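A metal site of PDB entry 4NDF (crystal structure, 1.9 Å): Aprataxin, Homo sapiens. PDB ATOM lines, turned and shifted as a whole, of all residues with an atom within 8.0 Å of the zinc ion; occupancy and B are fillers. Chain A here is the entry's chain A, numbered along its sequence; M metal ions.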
ATOM      1  N   TRP A 119     -16.725  25.069 -15.500  1.00  0.00           N
ATOM      2  CA  TRP A 119     -15.688  25.960 -15.991  1.00  0.00           C
ATOM      3  C   TRP A 119     -16.046  26.606 -17.337  1.00  0.00           C
ATOM      4  O   TRP A 119     -15.974  27.813 -17.491  1.00  0.00           O
ATOM      5  CB  TRP A 119     -14.353  25.231 -16.124  1.00  0.00           C
ATOM      6  CG  TRP A 119     -13.286  26.136 -16.642  1.00  0.00           C
ATOM      7  CD1 TRP A 119     -12.789  26.178 -17.918  1.00  0.00           C
ATOM      8  CD2 TRP A 119     -12.608  27.162 -15.918  1.00  0.00           C
ATOM      9  NE1 TRP A 119     -11.843  27.160 -18.019  1.00  0.00           N
ATOM     10  CE2 TRP A 119     -11.715  27.788 -16.806  1.00  0.00           C
ATOM     11  CE3 TRP A 119     -12.678  27.613 -14.592  1.00  0.00           C
ATOM     12  CZ2 TRP A 119     -10.884  28.836 -16.410  1.00  0.00           C
ATOM     13  CZ3 TRP A 119     -11.846  28.655 -14.204  1.00  0.00           C
ATOM     14  CH2 TRP A 119     -10.966  29.256 -15.112  1.00  0.00           C
ATOM     15  N   ARG A 158      -8.957  25.519 -20.078  1.00  0.00           N
ATOM     16  CA  ARG A 158      -8.018  26.584 -20.413  1.00  0.00           C
ATOM     17  C   ARG A 158      -8.218  27.735 -19.451  1.00  0.00           C
ATOM     18  O   ARG A 158      -9.334  28.212 -19.253  1.00  0.00           O
ATOM     19  CB  ARG A 158      -8.230  27.069 -21.855  1.00  0.00           C
ATOM     20  CG  ARG A 158      -7.203  28.102 -22.303  1.00  0.00           C
ATOM     21  CD  ARG A 158      -7.568  28.769 -23.614  1.00  0.00           C
ATOM     22  NE  ARG A 158      -7.579  27.840 -24.737  1.00  0.00           N
ATOM     23  CZ  ARG A 158      -6.505  27.465 -25.427  1.00  0.00           C
ATOM     24  NH1 ARG A 158      -5.309  27.946 -25.094  1.00  0.00           N
ATOM     25  NH2 ARG A 158      -6.626  26.613 -26.424  1.00  0.00           N
ATOM     26  N   CYS A 159      -7.121  28.181 -18.843  1.00  0.00           N
ATOM     27  CA  CYS A 159      -7.152  29.306 -17.912  1.00  0.00           C
ATOM     28  C   CYS A 159      -7.644  30.573 -18.615  1.00  0.00           C
ATOM     29  O   CYS A 159      -7.220  30.879 -19.735  1.00  0.00           O
ATOM     30  CB  CYS A 159      -5.774  29.530 -17.290  1.00  0.00           C
ATOM     31  SG  CYS A 159      -5.681  30.979 -16.216  1.00  0.00           S
ATOM     32  N   HIS A 160      -8.517  31.308 -17.936  1.00  0.00           N
ATOM     33  CA  HIS A 160      -9.072  32.549 -18.480  1.00  0.00           C
ATOM     34  C   HIS A 160      -8.085  33.716 -18.408  1.00  0.00           C
ATOM     35  O   HIS A 160      -8.278  34.729 -19.064  1.00  0.00           O
ATOM     36  CB  HIS A 160     -10.352  32.913 -17.714  1.00  0.00           C
ATOM     37  CG  HIS A 160     -10.134  33.202 -16.264  1.00  0.00           C
ATOM     38  ND1 HIS A 160      -9.396  32.391 -15.437  1.00  0.00           N
ATOM     39  CD2 HIS A 160     -10.570  34.231 -15.483  1.00  0.00           C
ATOM     40  CE1 HIS A 160      -9.381  32.900 -14.216  1.00  0.00           C
ATOM     41  NE2 HIS A 160     -10.088  34.019 -14.225  1.00  0.00           N
ATOM     42  N   GLU A 161      -7.044  33.570 -17.597  1.00  0.00           N
ATOM     43  CA  GLU A 161      -6.086  34.652 -17.362  1.00  0.00           C
ATOM     44  C   GLU A 161      -4.897  34.616 -18.326  1.00  0.00           C
ATOM     45  O   GLU A 161      -4.499  35.648 -18.868  1.00  0.00           O
ATOM     46  CB  GLU A 161      -5.587  34.639 -15.918  1.00  0.00           C
ATOM     47  CG  GLU A 161      -6.663  34.875 -14.873  1.00  0.00           C
ATOM     48  CD  GLU A 161      -7.208  36.292 -14.891  1.00  0.00           C
ATOM     49  OE1 GLU A 161      -6.537  37.185 -15.457  1.00  0.00           O
ATOM     50  OE2 GLU A 161      -8.307  36.510 -14.331  1.00  0.00           O
ATOM     51  N   CYS A 162      -4.315  33.428 -18.511  1.00  0.00           N
ATOM     52  CA  CYS A 162      -3.075  33.296 -19.267  1.00  0.00           C
ATOM     53  C   CYS A 162      -3.157  32.289 -20.404  1.00  0.00           C
ATOM     54  O   CYS A 162      -2.160  32.014 -21.071  1.00  0.00           O
ATOM     55  CB  CYS A 162      -1.932  32.910 -18.329  1.00  0.00           C
ATOM     56  SG  CYS A 162      -2.023  31.211 -17.717  1.00  0.00           S
ATOM     57  N   GLN A 163      -4.349  31.722 -20.598  1.00  0.00           N
ATOM     58  CA  GLN A 163      -4.647  30.818 -21.714  1.00  0.00           C
ATOM     59  C   GLN A 163      -3.967  29.445 -21.643  1.00  0.00           C
ATOM     60  O   GLN A 163      -4.118  28.640 -22.563  1.00  0.00           O
ATOM     61  CB  GLN A 163      -4.350  31.490 -23.071  1.00  0.00           C
ATOM     62  CG  GLN A 163      -5.373  32.529 -23.502  1.00  0.00           C
ATOM     63  CD  GLN A 163      -5.363  33.774 -22.628  1.00  0.00           C
ATOM     64  OE1 GLN A 163      -4.399  34.552 -22.642  1.00  0.00           O
ATOM     65  NE2 GLN A 163      -6.424  33.968 -21.846  1.00  0.00           N
ATOM     66  N   GLN A 164      -3.233  29.173 -20.570  1.00  0.00           N
ATOM     67  CA  GLN A 164      -2.587  27.870 -20.417  1.00  0.00           C
ATOM     68  C   GLN A 164      -3.607  26.736 -20.343  1.00  0.00           C
ATOM     69  O   GLN A 164      -4.650  26.864 -19.706  1.00  0.00           O
ATOM     70  CB  GLN A 164      -1.660  27.843 -19.189  1.00  0.00           C
ATOM     71  CG  GLN A 164      -0.860  26.562 -19.044  1.00  0.00           C
ATOM     72  CD  GLN A 164       0.155  26.621 -17.903  1.00  0.00           C
ATOM     73  OE1 GLN A 164       0.636  27.692 -17.545  1.00  0.00           O
ATOM     74  NE2 GLN A 164       0.470  25.468 -17.325  1.00  0.00           N
ATOM     75  N   LEU A 165      -3.302  25.627 -21.017  1.00  0.00           N
ATOM     76  CA  LEU A 165      -4.168  24.453 -21.002  1.00  0.00           C
ATOM     77  C   LEU A 165      -3.851  23.567 -19.804  1.00  0.00           C
ATOM     78  O   LEU A 165      -2.690  23.276 -19.539  1.00  0.00           O
ATOM     79  CB  LEU A 165      -4.019  23.663 -22.315  1.00  0.00           C
ATOM     80  CG  LEU A 165      -4.505  24.426 -23.562  1.00  0.00           C
ATOM     81  CD1 LEU A 165      -4.186  23.672 -24.853  1.00  0.00           C
ATOM     82  CD2 LEU A 165      -5.999  24.709 -23.457  1.00  0.00           C
ATOM     83  N   LEU A 166      -4.890  23.164 -19.087  1.00  0.00           N
ATOM     84  CA  LEU A 166      -4.715  22.335 -17.887  1.00  0.00           C
ATOM     85  C   LEU A 166      -5.389  20.985 -18.104  1.00  0.00           C
ATOM     86  O   LEU A 166      -6.449  20.904 -18.726  1.00  0.00           O
ATOM     87  CB  LEU A 166      -5.277  23.039 -16.651  1.00  0.00           C
ATOM     88  CG  LEU A 166      -4.421  24.128 -15.973  1.00  0.00           C
ATOM     89  CD1 LEU A 166      -3.071  23.577 -15.539  1.00  0.00           C
ATOM     90  CD2 LEU A 166      -4.243  25.360 -16.850  1.00  0.00           C
ATOM     91  N   LEU A 172      -6.191  22.617 -12.473  1.00  0.00           N
ATOM     92  CA  LEU A 172      -6.653  23.945 -12.815  1.00  0.00           C
ATOM     93  C   LEU A 172      -6.853  24.805 -11.560  1.00  0.00           C
ATOM     94  O   LEU A 172      -6.434  25.958 -11.521  1.00  0.00           O
ATOM     95  CB  LEU A 172      -7.957  23.883 -13.628  1.00  0.00           C
ATOM     96  CG  LEU A 172      -8.645  25.241 -13.865  1.00  0.00           C
ATOM     97  CD1 LEU A 172      -7.709  26.208 -14.577  1.00  0.00           C
ATOM     98  CD2 LEU A 172      -9.924  25.038 -14.653  1.00  0.00           C
ATOM     99  N   HIS A 175      -3.520  25.847 -10.421  1.00  0.00           N
ATOM    100  CA  HIS A 175      -2.963  26.856 -11.317  1.00  0.00           C
ATOM    101  C   HIS A 175      -3.551  28.238 -11.026  1.00  0.00           C
ATOM    102  O   HIS A 175      -2.826  29.239 -11.067  1.00  0.00           O
ATOM    103  CB  HIS A 175      -3.205  26.471 -12.773  1.00  0.00           C
ATOM    104  CG  HIS A 175      -2.861  27.550 -13.754  1.00  0.00           C
ATOM    105  ND1 HIS A 175      -1.609  27.685 -14.307  1.00  0.00           N
ATOM    106  CD2 HIS A 175      -3.619  28.558 -14.272  1.00  0.00           C
ATOM    107  CE1 HIS A 175      -1.603  28.730 -15.131  1.00  0.00           C
ATOM    108  NE2 HIS A 175      -2.805  29.267 -15.122  1.00  0.00           N
ATOM    109  N   LEU A 176      -4.849  28.273 -10.751  1.00  0.00           N
ATOM    110  CA  LEU A 176      -5.559  29.532 -10.535  1.00  0.00           C
ATOM    111  C   LEU A 176      -4.986  30.332  -9.366  1.00  0.00           C
ATOM    112  O   LEU A 176      -5.032  31.565  -9.373  1.00  0.00           O
ATOM    113  CB  LEU A 176      -7.052  29.281 -10.320  1.00  0.00           C
ATOM    114  CG  LEU A 176      -7.850  28.807 -11.529  1.00  0.00           C
ATOM    115  CD1 LEU A 176      -9.256  28.419 -11.121  1.00  0.00           C
ATOM    116  CD2 LEU A 176      -7.881  29.874 -12.628  1.00  0.00           C
ATOM    117  N   ARG A 177      -4.447  29.626  -8.378  1.00  0.00           N
ATOM    118  CA  ARG A 177      -3.861  30.269  -7.197  1.00  0.00           C
ATOM    119  C   ARG A 177      -2.841  31.334  -7.579  1.00  0.00           C
ATOM    120  O   ARG A 177      -2.712  32.349  -6.904  1.00  0.00           O
ATOM    121  CB  ARG A 177      -3.211  29.230  -6.283  1.00  0.00           C
ATOM    122  CG  ARG A 177      -4.193  28.291  -5.601  1.00  0.00           C
ATOM    123  CD  ARG A 177      -3.456  27.326  -4.681  1.00  0.00           C
ATOM    124  NE  ARG A 177      -4.268  26.957  -3.519  1.00  0.00           N
ATOM    125  CZ  ARG A 177      -4.238  27.603  -2.359  1.00  0.00           C
ATOM    126  NH1 ARG A 177      -3.443  28.655  -2.206  1.00  0.00           N
ATOM    127  NH2 ARG A 177      -5.012  27.208  -1.349  1.00  0.00           N
ATOM    128  N   LYS A 178      -2.120  31.094  -8.678  1.00  0.00           N
ATOM    129  CA  LYS A 178      -1.047  31.999  -9.083  1.00  0.00           C
ATOM    130  C   LYS A 178      -1.570  33.347  -9.603  1.00  0.00           C
ATOM    131  O   LYS A 178      -0.811  34.290  -9.765  1.00  0.00           O
ATOM    132  CB  LYS A 178      -0.142  31.351 -10.150  1.00  0.00           C
ATOM    133  CG  LYS A 178      -0.623  31.524 -11.593  1.00  0.00           C
ATOM    134  CD  LYS A 178       0.555  31.537 -12.563  1.00  0.00           C
ATOM    135  CE  LYS A 178       1.189  30.159 -12.700  1.00  0.00           C
ATOM    136  NZ  LYS A 178       2.509  30.241 -13.391  1.00  0.00           N
ATOM    137  N   HIS A 179      -2.873  33.422  -9.853  1.00  0.00           N
ATOM    138  CA  HIS A 179      -3.465  34.656 -10.352  1.00  0.00           C
ATOM    139  C   HIS A 179      -4.208  35.417  -9.256  1.00  0.00           C
ATOM    140  O   HIS A 179      -5.068  36.245  -9.540  1.00  0.00           O
ATOM    141  CB  HIS A 179      -4.415  34.367 -11.530  1.00  0.00           C
ATOM    142  CG  HIS A 179      -3.738  33.769 -12.718  1.00  0.00           C
ATOM    143  ND1 HIS A 179      -2.580  34.290 -13.262  1.00  0.00           N
ATOM    144  CD2 HIS A 179      -4.073  32.710 -13.494  1.00  0.00           C
ATOM    145  CE1 HIS A 179      -2.224  33.563 -14.311  1.00  0.00           C
ATOM    146  NE2 HIS A 179      -3.110  32.597 -14.471  1.00  0.00           N
HETATM  147 ZN    ZN M   1      -3.358  31.089 -15.864  1.00  0.00          ZN
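N of Gln 164 sits close to SG of Cys 162 (3.7 Å).
The backbone NH of Glu 161 lies close to the side-chain sulfur of Cys 159, 3.2 Å away.
N of Cys 159 sits at hydrogen-bond distance from O of Gln 164.
Of the 16 residues printed, 4 come within 4 Å of the zinc ion.
Along chain A the residues within 4 Å of the zinc ion span positions 159 to 179.
The zinc ion is bound by NE2 of His 175 (2.0 Å), NE2 of His 179 (2.1 Å), SG of Cys 162 (2.3 Å) and SG of Cys 159 (2.4 Å).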
